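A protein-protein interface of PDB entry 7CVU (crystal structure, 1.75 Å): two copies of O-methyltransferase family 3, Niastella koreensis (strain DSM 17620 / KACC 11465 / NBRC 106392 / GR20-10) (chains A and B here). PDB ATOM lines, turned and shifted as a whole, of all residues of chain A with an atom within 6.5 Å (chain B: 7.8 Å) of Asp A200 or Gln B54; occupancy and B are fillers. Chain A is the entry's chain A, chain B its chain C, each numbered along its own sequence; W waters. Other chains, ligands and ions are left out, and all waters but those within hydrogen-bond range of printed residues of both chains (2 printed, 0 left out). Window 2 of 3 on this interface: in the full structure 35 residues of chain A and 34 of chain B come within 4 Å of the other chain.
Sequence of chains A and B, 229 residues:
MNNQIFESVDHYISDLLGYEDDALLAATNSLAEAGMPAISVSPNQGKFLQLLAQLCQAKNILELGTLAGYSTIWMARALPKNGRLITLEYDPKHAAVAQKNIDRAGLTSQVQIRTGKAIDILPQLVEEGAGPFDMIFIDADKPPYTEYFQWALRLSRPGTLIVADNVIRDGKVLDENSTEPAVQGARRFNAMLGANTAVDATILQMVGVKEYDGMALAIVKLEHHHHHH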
ATOM      1  N   GLY A 159      28.491 -35.708  25.640  1.00  0.00           N
ATOM      2  CA  GLY A 159      27.294 -34.846  25.602  1.00  0.00           C
ATOM      3  C   GLY A 159      27.130 -33.978  26.827  1.00  0.00           C
ATOM      4  O   GLY A 159      26.190 -33.206  26.826  1.00  0.00           O
ATOM      5  N   ASN A 196      41.213 -26.903  22.426  1.00  0.00           N
ATOM      6  CA  ASN A 196      40.762 -28.178  23.030  1.00  0.00           C
ATOM      7  C   ASN A 196      39.909 -28.973  22.018  1.00  0.00           C
ATOM      8  O   ASN A 196      38.975 -28.394  21.408  1.00  0.00           O
ATOM      9  CB  ASN A 196      40.003 -27.900  24.313  1.00  0.00           C
ATOM     10  CG  ASN A 196      39.657 -29.167  25.058  1.00  0.00           C
ATOM     11  OD1 ASN A 196      38.871 -29.959  24.569  1.00  0.00           O
ATOM     12  ND2 ASN A 196      40.198 -29.347  26.258  1.00  0.00           N
ATOM     13  N   THR A 197      40.233 -30.260  21.841  1.00  0.00           N
ATOM     14  CA  THR A 197      39.557 -31.146  20.854  1.00  0.00           C
ATOM     15  C   THR A 197      38.759 -32.239  21.574  1.00  0.00           C
ATOM     16  O   THR A 197      38.193 -33.088  20.851  1.00  0.00           O
ATOM     17  CB  THR A 197      40.530 -31.661  19.787  1.00  0.00           C
ATOM     18  OG1 THR A 197      41.498 -32.514  20.385  1.00  0.00           O
ATOM     19  CG2 THR A 197      41.175 -30.550  18.996  1.00  0.00           C
ATOM     20  N   ALA A 198      38.669 -32.220  22.897  1.00  0.00           N
ATOM     21  CA  ALA A 198      37.771 -33.066  23.709  1.00  0.00           C
ATOM     22  C   ALA A 198      36.370 -32.432  23.742  1.00  0.00           C
ATOM     23  O   ALA A 198      35.476 -33.108  24.231  1.00  0.00           O
ATOM     24  CB  ALA A 198      38.283 -33.158  25.128  1.00  0.00           C
ATOM     25  N   VAL A 199      36.228 -31.149  23.387  1.00  0.00           N
ATOM     26  CA  VAL A 199      34.941 -30.400  23.438  1.00  0.00           C
ATOM     27  C   VAL A 199      34.724 -29.644  22.125  1.00  0.00           C
ATOM     28  O   VAL A 199      35.706 -29.334  21.431  1.00  0.00           O
ATOM     29  CB  VAL A 199      34.843 -29.422  24.615  1.00  0.00           C
ATOM     30  CG1 VAL A 199      35.065 -30.135  25.946  1.00  0.00           C
ATOM     31  CG2 VAL A 199      35.763 -28.212  24.454  1.00  0.00           C
ATOM     32  N   ASP A 200      33.450 -29.344  21.864  1.00  0.00           N
ATOM     33  CA  ASP A 200      33.031 -28.301  20.906  1.00  0.00           C
ATOM     34  C   ASP A 200      32.525 -27.126  21.731  1.00  0.00           C
ATOM     35  O   ASP A 200      31.800 -27.366  22.697  1.00  0.00           O
ATOM     36  CB  ASP A 200      31.948 -28.818  19.969  1.00  0.00           C
ATOM     37  CG  ASP A 200      32.449 -29.942  19.094  1.00  0.00           C
ATOM     38  OD1 ASP A 200      33.535 -29.751  18.470  1.00  0.00           O
ATOM     39  OD2 ASP A 200      31.775 -31.004  19.070  1.00  0.00           O
ATOM     40  N   ALA A 201      32.944 -25.905  21.417  1.00  0.00           N
ATOM     41  CA  ALA A 201      32.633 -24.766  22.309  1.00  0.00           C
ATOM     42  C   ALA A 201      32.450 -23.431  21.589  1.00  0.00           C
ATOM     43  O   ALA A 201      32.841 -23.268  20.414  1.00  0.00           O
ATOM     44  CB  ALA A 201      33.725 -24.666  23.380  1.00  0.00           C
ATOM     45  N   THR A 202      31.818 -22.513  22.304  1.00  0.00           N
ATOM     46  CA  THR A 202      31.722 -21.081  21.950  1.00  0.00           C
ATOM     47  C   THR A 202      31.803 -20.230  23.207  1.00  0.00           C
ATOM     48  O   THR A 202      31.766 -20.751  24.340  1.00  0.00           O
ATOM     49  CB  THR A 202      30.454 -20.804  21.115  1.00  0.00           C
ATOM     50  OG1 THR A 202      30.582 -19.518  20.477  1.00  0.00           O
ATOM     51  CG2 THR A 202      29.186 -20.869  21.948  1.00  0.00           C
ATOM     52  N   LEU A 217      30.432 -21.936  26.602  1.00  0.00           N
ATOM     53  CA  LEU A 217      29.597 -23.164  26.559  1.00  0.00           C
ATOM     54  C   LEU A 217      30.400 -24.240  25.820  1.00  0.00           C
ATOM     55  O   LEU A 217      30.920 -23.956  24.723  1.00  0.00           O
ATOM     56  CB  LEU A 217      28.315 -22.923  25.771  1.00  0.00           C
ATOM     57  CG  LEU A 217      27.345 -21.873  26.263  1.00  0.00           C
ATOM     58  CD1 LEU A 217      26.141 -21.834  25.323  1.00  0.00           C
ATOM     59  CD2 LEU A 217      26.877 -22.140  27.653  1.00  0.00           C
ATOM     60  N   ALA A 218      30.549 -25.399  26.428  1.00  0.00           N
ATOM     61  CA  ALA A 218      31.378 -26.468  25.838  1.00  0.00           C
ATOM     62  C   ALA A 218      30.582 -27.773  25.949  1.00  0.00           C
ATOM     63  O   ALA A 218      30.030 -28.080  27.035  1.00  0.00           O
ATOM     64  CB  ALA A 218      32.731 -26.567  26.498  1.00  0.00           C
ATOM     65  N   ILE A 219      30.499 -28.508  24.851  1.00  0.00           N
ATOM     66  CA  ILE A 219      29.908 -29.880  24.831  1.00  0.00           C
ATOM     67  C   ILE A 219      31.018 -30.920  24.709  1.00  0.00           C
ATOM     68  O   ILE A 219      31.872 -30.870  23.795  1.00  0.00           O
ATOM     69  CB  ILE A 219      28.840 -30.066  23.748  1.00  0.00           C
ATOM     70  CG1 ILE A 219      27.742 -29.014  23.899  1.00  0.00           C
ATOM     71  CG2 ILE A 219      28.261 -31.470  23.786  1.00  0.00           C
ATOM     72  CD1 ILE A 219      26.798 -28.975  22.740  1.00  0.00           C
ATOM     73  N   VAL A 220      30.966 -31.875  25.614  1.00  0.00           N
ATOM     74  CA  VAL A 220      31.982 -32.955  25.685  1.00  0.00           C
ATOM     75  C   VAL A 220      31.739 -33.952  24.528  1.00  0.00           C
ATOM     76  O   VAL A 220      30.626 -34.460  24.358  1.00  0.00           O
ATOM     77  CB  VAL A 220      31.969 -33.609  27.085  1.00  0.00           C
ATOM     78  CG1 VAL A 220      32.957 -34.778  27.131  1.00  0.00           C
ATOM     79  CG2 VAL A 220      32.235 -32.601  28.205  1.00  0.00           C
ATOM     80  N   LYS A 221      32.782 -34.245  23.747  1.00  0.00           N
ATOM     81  CA  LYS A 221      32.684 -35.074  22.540  1.00  0.00           C
ATOM     82  C   LYS A 221      32.804 -36.541  22.951  1.00  0.00           C
ATOM     83  O   LYS A 221      33.453 -36.856  23.946  1.00  0.00           O
ATOM     84  CB  LYS A 221      33.773 -34.679  21.544  1.00  0.00           C
ATOM     85  CG  LYS A 221      33.587 -33.306  20.930  1.00  0.00           C
ATOM     86  CD  LYS A 221      34.860 -32.814  20.282  1.00  0.00           C
ATOM     87  CE  LYS A 221      35.246 -33.553  19.032  1.00  0.00           C
ATOM     88  NZ  LYS A 221      36.580 -33.107  18.556  1.00  0.00           N
ATOM     89  N   LEU B  17      37.162 -19.967  18.169  1.00  0.00           N
ATOM     90  CA  LEU B  17      36.020 -20.910  18.373  1.00  0.00           C
ATOM     91  C   LEU B  17      34.968 -20.790  17.282  1.00  0.00           C
ATOM     92  O   LEU B  17      33.865 -21.359  17.483  1.00  0.00           O
ATOM     93  CB  LEU B  17      35.381 -20.720  19.755  1.00  0.00           C
ATOM     94  CG  LEU B  17      36.243 -21.191  20.922  1.00  0.00           C
ATOM     95  CD1 LEU B  17      35.621 -20.849  22.248  1.00  0.00           C
ATOM     96  CD2 LEU B  17      36.427 -22.714  20.851  1.00  0.00           C
ATOM     97  N   GLY B  46      26.484 -19.134  14.111  1.00  0.00           N
ATOM     98  CA  GLY B  46      26.442 -20.472  13.509  1.00  0.00           C
ATOM     99  C   GLY B  46      26.972 -21.544  14.438  1.00  0.00           C
ATOM    100  O   GLY B  46      26.361 -22.579  14.521  1.00  0.00           O
ATOM    101  N   LYS B  47      28.109 -21.319  15.071  1.00  0.00           N
ATOM    102  CA  LYS B  47      28.675 -22.246  16.067  1.00  0.00           C
ATOM    103  C   LYS B  47      27.657 -22.457  17.206  1.00  0.00           C
ATOM    104  O   LYS B  47      27.455 -23.620  17.613  1.00  0.00           O
ATOM    105  CB  LYS B  47      30.025 -21.741  16.581  1.00  0.00           C
ATOM    106  CG  LYS B  47      30.745 -22.699  17.493  1.00  0.00           C
ATOM    107  CD  LYS B  47      31.181 -23.988  16.842  1.00  0.00           C
ATOM    108  CE  LYS B  47      32.123 -24.786  17.733  1.00  0.00           C
ATOM    109  NZ  LYS B  47      33.489 -24.219  17.785  1.00  0.00           N
ATOM    110  N   PHE B  48      27.028 -21.396  17.705  1.00  0.00           N
ATOM    111  CA  PHE B  48      26.012 -21.536  18.788  1.00  0.00           C
ATOM    112  C   PHE B  48      24.864 -22.433  18.312  1.00  0.00           C
ATOM    113  O   PHE B  48      24.441 -23.342  19.065  1.00  0.00           O
ATOM    114  CB  PHE B  48      25.615 -20.150  19.283  1.00  0.00           C
ATOM    115  CG  PHE B  48      24.589 -20.142  20.371  1.00  0.00           C
ATOM    116  CD1 PHE B  48      24.704 -20.977  21.482  1.00  0.00           C
ATOM    117  CD2 PHE B  48      23.562 -19.219  20.322  1.00  0.00           C
ATOM    118  CE1 PHE B  48      23.772 -20.918  22.497  1.00  0.00           C
ATOM    119  CE2 PHE B  48      22.632 -19.159  21.344  1.00  0.00           C
ATOM    120  CZ  PHE B  48      22.730 -20.018  22.408  1.00  0.00           C
ATOM    121  N   LEU B  49      24.326 -22.173  17.123  1.00  0.00           N
ATOM    122  CA  LEU B  49      23.230 -23.011  16.568  1.00  0.00           C
ATOM    123  C   LEU B  49      23.690 -24.466  16.439  1.00  0.00           C
ATOM    124  O   LEU B  49      22.916 -25.373  16.774  1.00  0.00           O
ATOM    125  CB  LEU B  49      22.728 -22.435  15.238  1.00  0.00           C
ATOM    126  CG  LEU B  49      22.057 -21.069  15.351  1.00  0.00           C
ATOM    127  CD1 LEU B  49      21.822 -20.475  13.981  1.00  0.00           C
ATOM    128  CD2 LEU B  49      20.766 -21.105  16.166  1.00  0.00           C
ATOM    129  N   GLN B  50      24.898 -24.689  15.957  1.00  0.00           N
ATOM    130  CA  GLN B  50      25.422 -26.049  15.798  1.00  0.00           C
ATOM    131  C   GLN B  50      25.448 -26.680  17.191  1.00  0.00           C
ATOM    132  O   GLN B  50      25.061 -27.830  17.326  1.00  0.00           O
ATOM    133  CB  GLN B  50      26.780 -25.983  15.112  1.00  0.00           C
ATOM    134  CG  GLN B  50      27.378 -27.354  14.801  1.00  0.00           C
ATOM    135  CD  GLN B  50      28.714 -27.183  14.112  1.00  0.00           C
ATOM    136  OE1 GLN B  50      29.763 -26.966  14.749  1.00  0.00           O
ATOM    137  NE2 GLN B  50      28.684 -27.165  12.793  1.00  0.00           N
ATOM    138  N   LEU B  51      25.944 -25.967  18.203  1.00  0.00           N
ATOM    139  CA  LEU B  51      26.099 -26.556  19.550  1.00  0.00           C
ATOM    140  C   LEU B  51      24.716 -26.879  20.147  1.00  0.00           C
ATOM    141  O   LEU B  51      24.550 -27.943  20.763  1.00  0.00           O
ATOM    142  CB  LEU B  51      26.857 -25.605  20.470  1.00  0.00           C
ATOM    143  CG  LEU B  51      28.333 -25.401  20.153  1.00  0.00           C
ATOM    144  CD1 LEU B  51      28.882 -24.292  21.046  1.00  0.00           C
ATOM    145  CD2 LEU B  51      29.132 -26.667  20.338  1.00  0.00           C
ATOM    146  N   LEU B  52      23.727 -26.037  19.909  1.00  0.00           N
ATOM    147  CA  LEU B  52      22.331 -26.327  20.334  1.00  0.00           C
ATOM    148  C   LEU B  52      21.847 -27.582  19.623  1.00  0.00           C
ATOM    149  O   LEU B  52      21.261 -28.436  20.293  1.00  0.00           O
ATOM    150  CB  LEU B  52      21.366 -25.169  20.100  1.00  0.00           C
ATOM    151  CG  LEU B  52      21.682 -23.933  20.928  1.00  0.00           C
ATOM    152  CD1 LEU B  52      20.942 -22.691  20.419  1.00  0.00           C
ATOM    153  CD2 LEU B  52      21.439 -24.204  22.413  1.00  0.00           C
ATOM    154  N   ALA B  53      22.063 -27.702  18.329  1.00  0.00           N
ATOM    155  CA  ALA B  53      21.665 -28.941  17.613  1.00  0.00           C
ATOM    156  C   ALA B  53      22.355 -30.160  18.241  1.00  0.00           C
ATOM    157  O   ALA B  53      21.710 -31.206  18.373  1.00  0.00           O
ATOM    158  CB  ALA B  53      21.965 -28.786  16.155  1.00  0.00           C
ATOM    159  N   GLN B  54      23.634 -30.041  18.577  1.00  0.00           N
ATOM    160  CA  GLN B  54      24.455 -31.154  19.147  1.00  0.00           C
ATOM    161  C   GLN B  54      23.901 -31.507  20.523  1.00  0.00           C
ATOM    162  O   GLN B  54      23.727 -32.713  20.793  1.00  0.00           O
ATOM    163  CB  GLN B  54      25.900 -30.721  19.273  1.00  0.00           C
ATOM    164  CG  GLN B  54      26.698 -30.742  18.003  1.00  0.00           C
ATOM    165  CD  GLN B  54      28.116 -30.361  18.363  1.00  0.00           C
ATOM    166  OE1 GLN B  54      28.724 -30.924  19.276  1.00  0.00           O
ATOM    167  NE2 GLN B  54      28.574 -29.261  17.815  1.00  0.00           N
ATOM    168  N   LEU B  55      23.566 -30.503  21.334  1.00  0.00           N
ATOM    169  CA  LEU B  55      23.020 -30.732  22.691  1.00  0.00           C
ATOM    170  C   LEU B  55      21.640 -31.431  22.594  1.00  0.00           C
ATOM    171  O   LEU B  55      21.396 -32.345  23.394  1.00  0.00           O
ATOM    172  CB  LEU B  55      22.968 -29.366  23.376  1.00  0.00           C
ATOM    173  CG  LEU B  55      22.705 -29.396  24.864  1.00  0.00           C
ATOM    174  CD1 LEU B  55      23.780 -30.202  25.587  1.00  0.00           C
ATOM    175  CD2 LEU B  55      22.619 -27.962  25.355  1.00  0.00           C
ATOM    176  N   CYS B  56      20.809 -31.085  21.606  1.00  0.00           N
ATOM    177  CA  CYS B  56      19.499 -31.724  21.300  1.00  0.00           C
ATOM    178  C   CYS B  56      19.701 -33.156  20.741  1.00  0.00           C
ATOM    179  O   CYS B  56      18.685 -33.810  20.488  1.00  0.00           O
ATOM    180  CB  CYS B  56      18.689 -30.858  20.318  1.00  0.00           C
ATOM    181  SG  CYS B  56      18.090 -29.307  21.046  1.00  0.00           S
ATOM    182  N   GLN B  57      20.916 -33.553  20.309  1.00  0.00           N
ATOM    183  CA  GLN B  57      21.128 -34.834  19.581  1.00  0.00           C
ATOM    184  C   GLN B  57      20.156 -34.822  18.397  1.00  0.00           C
ATOM    185  O   GLN B  57      19.554 -35.834  18.089  1.00  0.00           O
ATOM    186  CB  GLN B  57      20.985 -36.028  20.526  1.00  0.00           C
ATOM    187  CG  GLN B  57      21.869 -35.886  21.770  1.00  0.00           C
ATOM    188  CD  GLN B  57      22.138 -37.146  22.567  1.00  0.00           C
ATOM    189  OE1 GLN B  57      21.820 -37.252  23.765  1.00  0.00           O
ATOM    190  NE2 GLN B  57      22.807 -38.092  21.926  1.00  0.00           N
ATOM    191  N   ALA B  58      20.049 -33.675  17.724  1.00  0.00           N
ATOM    192  CA  ALA B  58      19.095 -33.463  16.614  1.00  0.00           C
ATOM    193  C   ALA B  58      19.355 -34.446  15.451  1.00  0.00           C
ATOM    194  O   ALA B  58      20.508 -34.605  14.954  1.00  0.00           O
ATOM    195  CB  ALA B  58      19.165 -32.019  16.175  1.00  0.00           C
ATOM    196  N   ILE B  61      15.784 -31.339  11.709  1.00  0.00           N
ATOM    197  CA  ILE B  61      15.817 -29.877  11.963  1.00  0.00           C
ATOM    198  C   ILE B  61      14.932 -29.181  10.920  1.00  0.00           C
ATOM    199  O   ILE B  61      14.979 -29.596   9.736  1.00  0.00           O
ATOM    200  CB  ILE B  61      17.269 -29.371  11.909  1.00  0.00           C
ATOM    201  CG1 ILE B  61      18.129 -30.040  12.989  1.00  0.00           C
ATOM    202  CG2 ILE B  61      17.284 -27.851  12.031  1.00  0.00           C
ATOM    203  CD1 ILE B  61      19.602 -29.773  12.837  1.00  0.00           C
ATOM    204  N   TRP B  74      25.885 -24.712   9.028  1.00  0.00           N
ATOM    205  CA  TRP B  74      26.230 -24.842  10.458  1.00  0.00           C
ATOM    206  C   TRP B  74      25.354 -25.920  11.130  1.00  0.00           C
ATOM    207  O   TRP B  74      25.921 -26.838  11.753  1.00  0.00           O
ATOM    208  CB  TRP B  74      26.120 -23.493  11.170  1.00  0.00           C
ATOM    209  CG  TRP B  74      27.323 -22.616  11.032  1.00  0.00           C
ATOM    210  CD1 TRP B  74      27.423 -21.487  10.274  1.00  0.00           C
ATOM    211  CD2 TRP B  74      28.590 -22.746  11.717  1.00  0.00           C
ATOM    212  NE1 TRP B  74      28.649 -20.907  10.460  1.00  0.00           N
ATOM    213  CE2 TRP B  74      29.395 -21.656  11.305  1.00  0.00           C
ATOM    214  CE3 TRP B  74      29.140 -23.674  12.605  1.00  0.00           C
ATOM    215  CZ2 TRP B  74      30.700 -21.464  11.779  1.00  0.00           C
ATOM    216  CZ3 TRP B  74      30.417 -23.488  13.084  1.00  0.00           C
ATOM    217  CH2 TRP B  74      31.189 -22.406  12.659  1.00  0.00           C
ATOM    218  N   MET B  75      24.031 -25.823  11.001  1.00  0.00           N
ATOM    219  CA  MET B  75      23.140 -26.738  11.753  1.00  0.00           C
ATOM    220  C   MET B  75      23.212 -28.166  11.148  1.00  0.00           C
ATOM    221  O   MET B  75      23.183 -29.148  11.920  1.00  0.00           O
ATOM    222  CB  MET B  75      21.727 -26.181  11.736  1.00  0.00           C
ATOM    223  CG  MET B  75      21.577 -24.898  12.603  1.00  0.00           C
ATOM    224  SD  MET B  75      19.828 -24.410  12.673  1.00  0.00           S
ATOM    225  CE  MET B  75      19.557 -23.821  11.003  1.00  0.00           C
ATOM    226  N   ARG B  77      25.538 -29.747   9.758  1.00  0.00           N
ATOM    227  CA  ARG B  77      26.801 -30.419  10.153  1.00  0.00           C
ATOM    228  C   ARG B  77      26.674 -31.107  11.518  1.00  0.00           C
ATOM    229  O   ARG B  77      27.560 -31.914  11.821  1.00  0.00           O
ATOM    230  CB  ARG B  77      27.926 -29.390  10.099  1.00  0.00           C
ATOM    231  CG  ARG B  77      28.433 -29.203   8.677  1.00  0.00           C
ATOM    232  CD  ARG B  77      29.386 -28.052   8.538  1.00  0.00           C
ATOM    233  NE  ARG B  77      29.962 -28.054   7.204  1.00  0.00           N
ATOM    234  CZ  ARG B  77      30.782 -27.129   6.763  1.00  0.00           C
ATOM    235  NH1 ARG B  77      31.144 -26.145   7.558  1.00  0.00           N
ATOM    236  NH2 ARG B  77      31.266 -27.219   5.529  1.00  0.00           N
ATOM    237  N   ALA B  78      25.645 -30.803  12.326  1.00  0.00           N
ATOM    238  CA  ALA B  78      25.396 -31.503  13.610  1.00  0.00           C
ATOM    239  C   ALA B  78      24.669 -32.836  13.408  1.00  0.00           C
ATOM    240  O   ALA B  78      24.606 -33.642  14.360  1.00  0.00           O
ATOM    241  CB  ALA B  78      24.648 -30.610  14.554  1.00  0.00           C
ATOM    242  N   LEU B  79      24.087 -33.073  12.230  1.00  0.00           N
ATOM    243  CA  LEU B  79      23.224 -34.242  12.031  1.00  0.00           C
ATOM    244  C   LEU B  79      23.994 -35.560  11.945  1.00  0.00           C
ATOM    245  O   LEU B  79      25.109 -35.644  11.477  1.00  0.00           O
ATOM    246  CB  LEU B  79      22.436 -34.061  10.738  1.00  0.00           C
ATOM    247  CG  LEU B  79      21.466 -32.888  10.704  1.00  0.00           C
ATOM    248  CD1 LEU B  79      21.062 -32.706   9.254  1.00  0.00           C
ATOM    249  CD2 LEU B  79      20.271 -33.153  11.586  1.00  0.00           C
ATOM    250  N   MET B 135      14.838 -29.731  16.621  1.00  0.00           N
ATOM    251  CA  MET B 135      15.241 -28.302  16.718  1.00  0.00           C
ATOM    252  C   MET B 135      14.604 -27.583  15.539  1.00  0.00           C
ATOM    253  O   MET B 135      14.620 -28.141  14.433  1.00  0.00           O
ATOM    254  CB  MET B 135      16.760 -28.131  16.706  1.00  0.00           C
ATOM    255  CG  MET B 135      17.198 -26.680  16.867  1.00  0.00           C
ATOM    256  SD  MET B 135      18.972 -26.597  17.049  1.00  0.00           S
ATOM    257  CE  MET B 135      19.244 -24.887  16.622  1.00  0.00           C
HETATM  258  O   HOH W   1      35.143 -25.874  19.488  1.00  0.00           O
HETATM  259  O   HOH W   2      31.992 -19.485  18.255  1.00  0.00           O
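The side-chain carboxylate of Asp A200 sits close to the side-chain amide oxygen of Gln B54 (3.1 Å).
NZ of Lys B47 lies within hydrogen-bond range of O of Ala A201 (2.9 Å).
O of Asp A200 sits at hydrogen-bond distance from N of Ile A219.
N of Leu A217 sits at hydrogen-bond distance from O of Thr A202.
The backbone carbonyl oxygen of Leu B17 sits at hydrogen-bond distance from the side-chain amino group of Lys B47, 2.9 Å away.
Among the printed residues, merely in contact across the chains: Ile A219 with Leu B51 (3.2 Å), Thr A202 with Leu B51 (3.6 Å), Asp A200 with Leu B51 (3.6 Å), Ala A201 with Leu B17 (3.6 Å), Ala A201 with Leu B51 (3.7 Å), Leu A217 with Phe B48 (3.8 Å), Ile A219 with Leu B55 (3.8 Å), Thr A202 with Leu B17 (3.9 Å) and Ile A219 with Gln B54 (3.98 Å).
Asp A200 touches just these residues of chain B: Leu B51 and Gln B54.
Of the printed residues of chain B, Thr A202 touches Leu B17 and Leu B51.
Printed residues of chain B within 4 Å of Leu A217: Phe B48 (3.8 Å).
Of the printed residues of chain A, Phe B48 touches Leu A217.
The nearest printed residue of chain A that does not touch Gln B54 is Lys A221 (5.7 Å).
The nearest printed residue of chain A that does not touch Phe B48 is Thr A202 (4.5 Å).
Of the 21 printed residues of chain B, 6 touch a printed residue of chain A.
Hydrophobic or aromatic side chains of chain B that line the printed part of chain A: Leu B17, Phe B48, Leu B51 and Leu B55.
Hydrophobic or aromatic side chains of chain A within 4 Å of the printed part of chain B: Leu A217 and Ile A219.
Among the printed residues, no Asp or Glu carboxylate lies within 4 Å of a Lys or Arg side-chain nitrogen of the other chain.
No position is printed for both chains.
Of the 11 pairs that touch across the chains among the printed residues, none has its exchanged pair printed and touching as well.
Water W2 bridges the side-chain hydroxyl (OG1) of Thr A202 (2.6 Å) and the backbone carbonyl oxygen (O) of Leu B17 (2.8 Å).
Water W1 bridges NZ of Lys B47 (2.9 Å) and N of Ala A201 (2.9 Å).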
